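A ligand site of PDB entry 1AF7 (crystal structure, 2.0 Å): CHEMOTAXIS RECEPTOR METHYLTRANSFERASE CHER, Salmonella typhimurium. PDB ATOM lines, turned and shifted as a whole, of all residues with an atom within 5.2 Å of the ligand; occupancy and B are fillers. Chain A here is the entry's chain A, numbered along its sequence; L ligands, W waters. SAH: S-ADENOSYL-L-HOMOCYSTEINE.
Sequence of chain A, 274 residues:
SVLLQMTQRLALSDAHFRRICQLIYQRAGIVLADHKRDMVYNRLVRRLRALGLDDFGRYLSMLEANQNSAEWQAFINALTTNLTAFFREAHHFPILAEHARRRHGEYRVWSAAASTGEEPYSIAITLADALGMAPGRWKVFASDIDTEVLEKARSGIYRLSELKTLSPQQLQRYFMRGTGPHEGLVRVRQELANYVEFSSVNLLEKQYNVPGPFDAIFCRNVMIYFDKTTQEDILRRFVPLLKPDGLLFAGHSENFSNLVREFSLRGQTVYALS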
ATOM      1  N   ALA A  28      13.034  21.299 -15.128  1.00  0.00           N
ATOM      2  CA  ALA A  28      12.996  19.847 -15.197  1.00  0.00           C
ATOM      3  C   ALA A  28      12.809  19.157 -13.866  1.00  0.00           C
ATOM      4  O   ALA A  28      12.763  17.922 -13.828  1.00  0.00           O
ATOM      5  CB  ALA A  28      14.271  19.336 -15.872  1.00  0.00           C
ATOM      6  N   GLY A  29      12.748  19.925 -12.778  1.00  0.00           N
ATOM      7  CA  GLY A  29      12.559  19.359 -11.453  1.00  0.00           C
ATOM      8  C   GLY A  29      13.794  18.692 -10.856  1.00  0.00           C
ATOM      9  O   GLY A  29      13.764  18.198  -9.726  1.00  0.00           O
ATOM     10  N   ILE A  30      14.870  18.689 -11.629  1.00  0.00           N
ATOM     11  CA  ILE A  30      16.131  18.088 -11.205  1.00  0.00           C
ATOM     12  C   ILE A  30      16.804  18.886 -10.104  1.00  0.00           C
ATOM     13  O   ILE A  30      16.993  20.099 -10.223  1.00  0.00           O
ATOM     14  CB  ILE A  30      17.100  17.965 -12.410  1.00  0.00           C
ATOM     15  CG1 ILE A  30      16.505  17.026 -13.464  1.00  0.00           C
ATOM     16  CG2 ILE A  30      18.452  17.445 -11.953  1.00  0.00           C
ATOM     17  CD1 ILE A  30      17.239  17.034 -14.778  1.00  0.00           C
ATOM     18  N   THR A  80      21.200  16.456 -17.259  1.00  0.00           N
ATOM     19  CA  THR A  80      20.506  15.258 -16.863  1.00  0.00           C
ATOM     20  C   THR A  80      21.541  14.153 -16.590  1.00  0.00           C
ATOM     21  O   THR A  80      22.701  14.264 -16.988  1.00  0.00           O
ATOM     22  CB  THR A  80      19.563  14.781 -17.974  1.00  0.00           C
ATOM     23  OG1 THR A  80      20.300  14.696 -19.187  1.00  0.00           O
ATOM     24  CG2 THR A  80      18.387  15.723 -18.156  1.00  0.00           C
ATOM     25  N   THR A  81      21.085  13.079 -15.933  1.00  0.00           N
ATOM     26  CA  THR A  81      21.891  11.911 -15.619  1.00  0.00           C
ATOM     27  C   THR A  81      21.166  10.734 -16.269  1.00  0.00           C
ATOM     28  O   THR A  81      20.068  10.348 -15.869  1.00  0.00           O
ATOM     29  CB  THR A  81      21.965  11.686 -14.104  1.00  0.00           C
ATOM     30  OG1 THR A  81      22.441  12.891 -13.483  1.00  0.00           O
ATOM     31  CG2 THR A  81      22.887  10.510 -13.777  1.00  0.00           C
ATOM     32  N   ASN A  82      21.820  10.134 -17.261  1.00  0.00           N
ATOM     33  CA  ASN A  82      21.236   9.063 -18.056  1.00  0.00           C
ATOM     34  C   ASN A  82      21.704   7.622 -17.833  1.00  0.00           C
ATOM     35  O   ASN A  82      21.422   6.771 -18.673  1.00  0.00           O
ATOM     36  CB  ASN A  82      21.450   9.391 -19.532  1.00  0.00           C
ATOM     37  CG  ASN A  82      21.246  10.848 -19.828  1.00  0.00           C
ATOM     38  OD1 ASN A  82      20.125  11.354 -19.842  1.00  0.00           O
ATOM     39  ND2 ASN A  82      22.331  11.548 -20.036  1.00  0.00           N
ATOM     40  N   LEU A  83      22.403   7.345 -16.741  1.00  0.00           N
ATOM     41  CA  LEU A  83      22.910   6.008 -16.484  1.00  0.00           C
ATOM     42  C   LEU A  83      21.809   4.938 -16.612  1.00  0.00           C
ATOM     43  O   LEU A  83      20.794   5.026 -15.926  1.00  0.00           O
ATOM     44  CB  LEU A  83      23.581   5.953 -15.115  1.00  0.00           C
ATOM     45  CG  LEU A  83      24.507   4.743 -14.890  1.00  0.00           C
ATOM     46  CD1 LEU A  83      25.534   4.648 -16.009  1.00  0.00           C
ATOM     47  CD2 LEU A  83      25.193   4.860 -13.523  1.00  0.00           C
ATOM     48  N   THR A  84      22.044   3.937 -17.441  1.00  0.00           N
ATOM     49  CA  THR A  84      21.062   2.876 -17.670  1.00  0.00           C
ATOM     50  C   THR A  84      21.766   1.643 -18.187  1.00  0.00           C
ATOM     51  O   THR A  84      22.976   1.662 -18.408  1.00  0.00           O
ATOM     52  CB  THR A  84      19.998   3.342 -18.715  1.00  0.00           C
ATOM     53  OG1 THR A  84      18.913   2.381 -18.815  1.00  0.00           O
ATOM     54  CG2 THR A  84      20.653   3.529 -20.079  1.00  0.00           C
ATOM     55  N   ALA A  85      21.005   0.576 -18.405  1.00  0.00           N
ATOM     56  CA  ALA A  85      21.536  -0.698 -18.888  1.00  0.00           C
ATOM     57  C   ALA A  85      20.416  -1.598 -19.408  1.00  0.00           C
ATOM     58  O   ALA A  85      19.269  -1.426 -19.041  1.00  0.00           O
ATOM     59  CB  ALA A  85      22.259  -1.420 -17.756  1.00  0.00           C
ATOM     60  N   ARG A  88      18.023  -3.911 -16.718  1.00  0.00           N
ATOM     61  CA  ARG A  88      18.367  -3.411 -15.392  1.00  0.00           C
ATOM     62  C   ARG A  88      17.154  -3.840 -14.547  1.00  0.00           C
ATOM     63  O   ARG A  88      16.051  -3.864 -15.079  1.00  0.00           O
ATOM     64  CB  ARG A  88      18.478  -1.881 -15.425  1.00  0.00           C
ATOM     65  CG  ARG A  88      19.023  -1.259 -14.164  1.00  0.00           C
ATOM     66  CD  ARG A  88      19.047   0.236 -14.248  1.00  0.00           C
ATOM     67  NE  ARG A  88      19.648   0.822 -13.047  1.00  0.00           N
ATOM     68  CZ  ARG A  88      19.973   2.098 -12.916  1.00  0.00           C
ATOM     69  NH1 ARG A  88      19.781   2.956 -13.904  1.00  0.00           N
ATOM     70  NH2 ARG A  88      20.484   2.531 -11.767  1.00  0.00           N
ATOM     71  N   ALA A 112       8.461   5.815 -19.122  1.00  0.00           N
ATOM     72  CA  ALA A 112       8.560   7.248 -18.807  1.00  0.00           C
ATOM     73  C   ALA A 112       9.961   7.882 -18.712  1.00  0.00           C
ATOM     74  O   ALA A 112      10.084   9.093 -18.625  1.00  0.00           O
ATOM     75  CB  ALA A 112       7.763   7.542 -17.564  1.00  0.00           C
ATOM     76  N   ALA A 113      11.012   7.073 -18.703  1.00  0.00           N
ATOM     77  CA  ALA A 113      12.368   7.608 -18.664  1.00  0.00           C
ATOM     78  C   ALA A 113      13.209   6.624 -19.437  1.00  0.00           C
ATOM     79  O   ALA A 113      13.915   5.812 -18.856  1.00  0.00           O
ATOM     80  CB  ALA A 113      12.863   7.719 -17.239  1.00  0.00           C
ATOM     81  N   ALA A 114      13.139   6.712 -20.762  1.00  0.00           N
ATOM     82  CA  ALA A 114      13.822   5.810 -21.683  1.00  0.00           C
ATOM     83  C   ALA A 114      15.332   5.882 -21.791  1.00  0.00           C
ATOM     84  O   ALA A 114      15.989   4.878 -22.129  1.00  0.00           O
ATOM     85  CB  ALA A 114      13.201   5.953 -23.082  1.00  0.00           C
ATOM     86  N   SER A 115      15.885   7.067 -21.534  1.00  0.00           N
ATOM     87  CA  SER A 115      17.300   7.328 -21.670  1.00  0.00           C
ATOM     88  C   SER A 115      17.732   6.942 -23.084  1.00  0.00           C
ATOM     89  O   SER A 115      17.034   7.273 -24.052  1.00  0.00           O
ATOM     90  CB  SER A 115      18.115   6.584 -20.619  1.00  0.00           C
ATOM     91  OG  SER A 115      19.459   7.022 -20.664  1.00  0.00           O
ATOM     92  N   GLU A 119      16.010   0.510 -21.673  1.00  0.00           N
ATOM     93  CA  GLU A 119      14.800   0.063 -20.992  1.00  0.00           C
ATOM     94  C   GLU A 119      13.666  -0.240 -21.996  1.00  0.00           C
ATOM     95  O   GLU A 119      13.064  -1.302 -21.904  1.00  0.00           O
ATOM     96  CB  GLU A 119      14.367   1.053 -19.920  1.00  0.00           C
ATOM     97  CG  GLU A 119      13.064   0.695 -19.232  1.00  0.00           C
ATOM     98  CD  GLU A 119      12.700   1.674 -18.169  1.00  0.00           C
ATOM     99  OE1 GLU A 119      13.366   1.642 -17.138  1.00  0.00           O
ATOM    100  OE2 GLU A 119      11.785   2.498 -18.377  1.00  0.00           O
ATOM    101  N   ASP A 144      11.485  10.758 -22.884  1.00  0.00           N
ATOM    102  CA  ASP A 144      12.511  11.278 -22.012  1.00  0.00           C
ATOM    103  C   ASP A 144      12.521  12.769 -22.280  1.00  0.00           C
ATOM    104  O   ASP A 144      12.023  13.207 -23.293  1.00  0.00           O
ATOM    105  CB  ASP A 144      13.865  10.685 -22.425  1.00  0.00           C
ATOM    106  CG  ASP A 144      14.916  10.809 -21.332  1.00  0.00           C
ATOM    107  OD1 ASP A 144      15.338  11.935 -21.014  1.00  0.00           O
ATOM    108  OD2 ASP A 144      15.302   9.782 -20.776  1.00  0.00           O
ATOM    109  N   ILE A 145      13.047  13.545 -21.364  1.00  0.00           N
ATOM    110  CA  ILE A 145      13.128  14.994 -21.543  1.00  0.00           C
ATOM    111  C   ILE A 145      14.383  15.394 -22.370  1.00  0.00           C
ATOM    112  O   ILE A 145      14.429  16.455 -22.986  1.00  0.00           O
ATOM    113  CB  ILE A 145      13.158  15.721 -20.176  1.00  0.00           C
ATOM    114  CG1 ILE A 145      12.921  17.221 -20.384  1.00  0.00           C
ATOM    115  CG2 ILE A 145      14.488  15.443 -19.434  1.00  0.00           C
ATOM    116  CD1 ILE A 145      13.104  18.046 -19.175  1.00  0.00           C
ATOM    117  N   ASP A 146      15.336  14.473 -22.424  1.00  0.00           N
ATOM    118  CA  ASP A 146      16.624  14.670 -23.087  1.00  0.00           C
ATOM    119  C   ASP A 146      16.556  14.156 -24.517  1.00  0.00           C
ATOM    120  O   ASP A 146      16.344  12.955 -24.772  1.00  0.00           O
ATOM    121  CB  ASP A 146      17.696  13.933 -22.258  1.00  0.00           C
ATOM    122  CG  ASP A 146      19.107  14.190 -22.706  1.00  0.00           C
ATOM    123  OD1 ASP A 146      19.397  14.255 -23.904  1.00  0.00           O
ATOM    124  OD2 ASP A 146      19.983  14.278 -21.841  1.00  0.00           O
ATOM    125  N   VAL A 149      19.848  11.697 -25.812  1.00  0.00           N
ATOM    126  CA  VAL A 149      19.664  10.277 -25.551  1.00  0.00           C
ATOM    127  C   VAL A 149      18.547   9.661 -26.406  1.00  0.00           C
ATOM    128  O   VAL A 149      18.645   8.500 -26.819  1.00  0.00           O
ATOM    129  CB  VAL A 149      19.444   9.988 -24.043  1.00  0.00           C
ATOM    130  CG1 VAL A 149      20.625  10.502 -23.238  1.00  0.00           C
ATOM    131  CG2 VAL A 149      18.120  10.579 -23.539  1.00  0.00           C
ATOM    132  N   VAL A 201       9.017  14.003 -23.539  1.00  0.00           N
ATOM    133  CA  VAL A 201       7.966  14.419 -22.632  1.00  0.00           C
ATOM    134  C   VAL A 201       8.670  14.807 -21.340  1.00  0.00           C
ATOM    135  O   VAL A 201       9.546  14.092 -20.875  1.00  0.00           O
ATOM    136  CB  VAL A 201       6.952  13.266 -22.370  1.00  0.00           C
ATOM    137  CG1 VAL A 201       5.907  13.722 -21.382  1.00  0.00           C
ATOM    138  CG2 VAL A 201       6.266  12.830 -23.680  1.00  0.00           C
ATOM    139  N   ASN A 202       8.359  15.989 -20.845  1.00  0.00           N
ATOM    140  CA  ASN A 202       8.940  16.477 -19.600  1.00  0.00           C
ATOM    141  C   ASN A 202       7.913  16.077 -18.543  1.00  0.00           C
ATOM    142  O   ASN A 202       6.741  16.439 -18.623  1.00  0.00           O
ATOM    143  CB  ASN A 202       9.108  18.006 -19.670  1.00  0.00           C
ATOM    144  CG  ASN A 202       9.630  18.606 -18.389  1.00  0.00           C
ATOM    145  OD1 ASN A 202       9.716  17.928 -17.366  1.00  0.00           O
ATOM    146  ND2 ASN A 202       9.964  19.873 -18.421  1.00  0.00           N
ATOM    147  N   LEU A 203       8.330  15.273 -17.582  1.00  0.00           N
ATOM    148  CA  LEU A 203       7.414  14.811 -16.559  1.00  0.00           C
ATOM    149  C   LEU A 203       6.756  15.907 -15.711  1.00  0.00           C
ATOM    150  O   LEU A 203       5.746  15.666 -15.068  1.00  0.00           O
ATOM    151  CB  LEU A 203       8.138  13.810 -15.658  1.00  0.00           C
ATOM    152  CG  LEU A 203       7.954  12.308 -15.871  1.00  0.00           C
ATOM    153  CD1 LEU A 203       7.519  12.009 -17.281  1.00  0.00           C
ATOM    154  CD2 LEU A 203       9.257  11.582 -15.462  1.00  0.00           C
ATOM    155  N   LEU A 204       7.341  17.107 -15.666  1.00  0.00           N
ATOM    156  CA  LEU A 204       6.741  18.180 -14.884  1.00  0.00           C
ATOM    157  C   LEU A 204       5.573  18.879 -15.594  1.00  0.00           C
ATOM    158  O   LEU A 204       5.035  19.850 -15.053  1.00  0.00           O
ATOM    159  CB  LEU A 204       7.782  19.226 -14.480  1.00  0.00           C
ATOM    160  CG  LEU A 204       8.816  18.961 -13.392  1.00  0.00           C
ATOM    161  CD1 LEU A 204       8.491  19.732 -12.145  1.00  0.00           C
ATOM    162  CD2 LEU A 204       8.938  17.488 -13.125  1.00  0.00           C
ATOM    163  N   ARG A 220      11.277   4.136 -13.766  1.00  0.00           N
ATOM    164  CA  ARG A 220      12.402   3.728 -12.958  1.00  0.00           C
ATOM    165  C   ARG A 220      13.613   4.622 -12.985  1.00  0.00           C
ATOM    166  O   ARG A 220      14.043   5.116 -14.035  1.00  0.00           O
ATOM    167  CB  ARG A 220      12.815   2.311 -13.343  1.00  0.00           C
ATOM    168  CG  ARG A 220      11.660   1.367 -13.533  1.00  0.00           C
ATOM    169  CD  ARG A 220      12.140  -0.074 -13.665  1.00  0.00           C
ATOM    170  NE  ARG A 220      13.069  -0.188 -14.769  1.00  0.00           N
ATOM    171  CZ  ARG A 220      13.635  -1.320 -15.158  1.00  0.00           C
ATOM    172  NH1 ARG A 220      13.381  -2.435 -14.514  1.00  0.00           N
ATOM    173  NH2 ARG A 220      14.505  -1.303 -16.154  1.00  0.00           N
ATOM    174  N   ASN A 221      14.186   4.815 -11.797  1.00  0.00           N
ATOM    175  CA  ASN A 221      15.402   5.593 -11.576  1.00  0.00           C
ATOM    176  C   ASN A 221      15.433   7.002 -12.127  1.00  0.00           C
ATOM    177  O   ASN A 221      16.412   7.408 -12.736  1.00  0.00           O
ATOM    178  CB  ASN A 221      16.597   4.773 -12.045  1.00  0.00           C
ATOM    179  CG  ASN A 221      16.676   3.428 -11.385  1.00  0.00           C
ATOM    180  OD1 ASN A 221      16.521   2.405 -12.019  1.00  0.00           O
ATOM    181  ND2 ASN A 221      16.831   3.429 -10.090  1.00  0.00           N
ATOM    182  N   VAL A 222      14.368   7.759 -11.905  1.00  0.00           N
ATOM    183  CA  VAL A 222      14.274   9.150 -12.356  1.00  0.00           C
ATOM    184  C   VAL A 222      13.698   9.991 -11.228  1.00  0.00           C
ATOM    185  O   VAL A 222      14.136  11.123 -10.995  1.00  0.00           O
ATOM    186  CB  VAL A 222      13.412   9.308 -13.638  1.00  0.00           C
ATOM    187  CG1 VAL A 222      12.067   8.620 -13.475  1.00  0.00           C
ATOM    188  CG2 VAL A 222      13.220  10.796 -13.967  1.00  0.00           C
ATOM    189  N   TYR A 225      15.877  12.036  -8.838  1.00  0.00           N
ATOM    190  CA  TYR A 225      16.438  13.355  -9.111  1.00  0.00           C
ATOM    191  C   TYR A 225      15.480  14.479  -8.739  1.00  0.00           C
ATOM    192  O   TYR A 225      15.838  15.649  -8.842  1.00  0.00           O
ATOM    193  CB  TYR A 225      16.781  13.496 -10.587  1.00  0.00           C
ATOM    194  CG  TYR A 225      17.720  12.426 -11.041  1.00  0.00           C
ATOM    195  CD1 TYR A 225      18.977  12.293 -10.464  1.00  0.00           C
ATOM    196  CD2 TYR A 225      17.346  11.499 -11.998  1.00  0.00           C
ATOM    197  CE1 TYR A 225      19.835  11.273 -10.828  1.00  0.00           C
ATOM    198  CE2 TYR A 225      18.199  10.461 -12.385  1.00  0.00           C
ATOM    199  CZ  TYR A 225      19.449  10.367 -11.791  1.00  0.00           C
ATOM    200  OH  TYR A 225      20.324   9.374 -12.182  1.00  0.00           O
ATOM    201  N   PHE A 226      14.266  14.112  -8.329  1.00  0.00           N
ATOM    202  CA  PHE A 226      13.235  15.069  -7.974  1.00  0.00           C
ATOM    203  C   PHE A 226      12.994  15.075  -6.475  1.00  0.00           C
ATOM    204  O   PHE A 226      13.472  14.193  -5.754  1.00  0.00           O
ATOM    205  CB  PHE A 226      11.903  14.701  -8.668  1.00  0.00           C
ATOM    206  CG  PHE A 226      12.002  14.537 -10.162  1.00  0.00           C
ATOM    207  CD1 PHE A 226      12.965  15.205 -10.895  1.00  0.00           C
ATOM    208  CD2 PHE A 226      11.105  13.711 -10.829  1.00  0.00           C
ATOM    209  CE1 PHE A 226      13.031  15.058 -12.274  1.00  0.00           C
ATOM    210  CE2 PHE A 226      11.170  13.553 -12.230  1.00  0.00           C
ATOM    211  CZ  PHE A 226      12.139  14.228 -12.949  1.00  0.00           C
HETATM  212  N   SAH L   1      14.597   4.130 -16.597  1.00  0.00           N
HETATM  213  CA  SAH L   1      15.970   3.829 -17.026  1.00  0.00           C
HETATM  214  CB  SAH L   1      16.721   5.132 -17.388  1.00  0.00           C
HETATM  215  CG  SAH L   1      16.953   6.059 -16.230  1.00  0.00           C
HETATM  216  SD  SAH L   1      17.991   7.540 -16.562  1.00  0.00           S
HETATM  217  C   SAH L   1      16.729   2.978 -15.967  1.00  0.00           C
HETATM  218  O   SAH L   1      16.071   2.536 -15.009  1.00  0.00           O
HETATM  219  OXT SAH L   1      17.709   2.315 -16.379  1.00  0.00           O
HETATM  220  C5' SAH L   1      16.802   8.755 -16.060  1.00  0.00           C
HETATM  221  C4' SAH L   1      16.302   9.615 -17.193  1.00  0.00           C
HETATM  222  O4' SAH L   1      15.268  10.494 -16.723  1.00  0.00           O
HETATM  223  C3' SAH L   1      17.379  10.524 -17.777  1.00  0.00           C
HETATM  224  O3' SAH L   1      17.809  10.009 -19.037  1.00  0.00           O
HETATM  225  C2' SAH L   1      16.728  11.906 -17.952  1.00  0.00           C
HETATM  226  O2' SAH L   1      16.860  12.509 -19.217  1.00  0.00           O
HETATM  227  C1' SAH L   1      15.276  11.652 -17.510  1.00  0.00           C
HETATM  228  N9  SAH L   1      14.599  12.748 -16.838  1.00  0.00           N
HETATM  229  C8  SAH L   1      15.091  13.580 -15.853  1.00  0.00           C
HETATM  230  N7  SAH L   1      14.256  14.523 -15.502  1.00  0.00           N
HETATM  231  C5  SAH L   1      13.135  14.308 -16.295  1.00  0.00           C
HETATM  232  C6  SAH L   1      11.928  15.002 -16.438  1.00  0.00           C
HETATM  233  N6  SAH L   1      11.627  16.105 -15.749  1.00  0.00           N
HETATM  234  N1  SAH L   1      11.028  14.530 -17.329  1.00  0.00           N
HETATM  235  C2  SAH L   1      11.341  13.432 -18.038  1.00  0.00           C
HETATM  236  N3  SAH L   1      12.460  12.696 -18.011  1.00  0.00           N
HETATM  237  C4  SAH L   1      13.331  13.199 -17.103  1.00  0.00           C
HETATM  238  O   HOH W   1      19.362   6.807 -13.504  1.00  0.00           O
HETATM  239  O   HOH W   2      11.327   4.495 -16.762  1.00  0.00           O
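An oxygen (O2') of the ligand lies within hydrogen-bond range of the side-chain carboxylate (OD1) of Asp 144 (2.4 Å). An oxygen (OXT) of the ligand lies within hydrogen-bond range of the side-chain hydroxyl of Thr 84 (2.7 Å). An oxygen (O3') of the ligand is in hydrogen-bond range of the side-chain amide oxygen (OD1) of Asn 82 (2.8 Å). O of Arg 220 sits at hydrogen-bond distance from N of the ligand, 2.8 Å away. The backbone NH (N) of Leu 203 is in hydrogen-bond range of a nitrogen (N1) of the ligand (2.8 Å). The side-chain carboxylate (OE1) of Glu 119 is in salt-bridge range of a nitrogen (N) of the ligand. N6 of the ligand lies within hydrogen-bond range of O of Ala 28 (2.9 Å). O of Ala 113 sits at hydrogen-bond distance from N of the ligand (2.9 Å). The side-chain amide oxygen (OD1) of Asn 221 lies close to an oxygen (O) of the ligand (3.0 Å). OD1 of Asn 202 is in hydrogen-bond range of N6 of the ligand, 3.1 Å away. An oxygen (OXT) of the ligand lies within salt-bridge range of the guanidinium group of Arg 88 (3.3 Å).
The backbone NH (N) of Val 201 sits at hydrogen-bond distance from the backbone carbonyl oxygen (O) of Asp 144 (3.1 Å). OD1 of Asp 144 lies within hydrogen-bond range of N of Asp 146 (2.9 Å). O of Asn 82 lies within hydrogen-bond range of OG of Ser 115 (2.8 Å). NH1 of Arg 220 is in hydrogen-bond range of O of Arg 88, at 3.1 Å. The side-chain amide oxygen (OD1) of Asn 202 is in hydrogen-bond range of the backbone NH (N) of Leu 204 (3.0 Å). O of Leu 83 sits at hydrogen-bond distance from NH1 of Arg 88 (3.1 Å). The side-chain hydroxyl (OG1) of Thr 80 is in hydrogen-bond range of the side-chain carboxylate (OD2) of Asp 146 (2.7 Å). N of Val 149 is in hydrogen-bond range of OD1 of Asp 146.
A sulfur (SD) of the ligand lies close to the backbone carbonyl oxygen of Thr 81 (3.6 Å). Merely in contact with the ligand: Ile 30 (3.9 Å), Thr 80 (3.7 Å), Leu 83 (3.8 Å), Ser 115 (3.8 Å), Ile 145 (3.4 Å), Asp 146 (3.5 Å), Val 201 (3.4 Å), Val 222 (3.4 Å) and Phe 226 (3.3 Å). Hydrophobic or aromatic side chains that line the ligand: Ile 30, Ala 113, Ile 145, Leu 203, Val 222 and Phe 226. The nearest printed residue that does not touch the ligand is Leu 204 (4.004 Å).
Water W2 lies within hydrogen-bond range of the side-chain carboxylate of Glu 119 (2.6 Å), the backbone NH of Arg 220 (3.0 Å), the backbone NH of Ala 113 (3.2 Å) and a nitrogen (N) of the ligand (3.3 Å).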
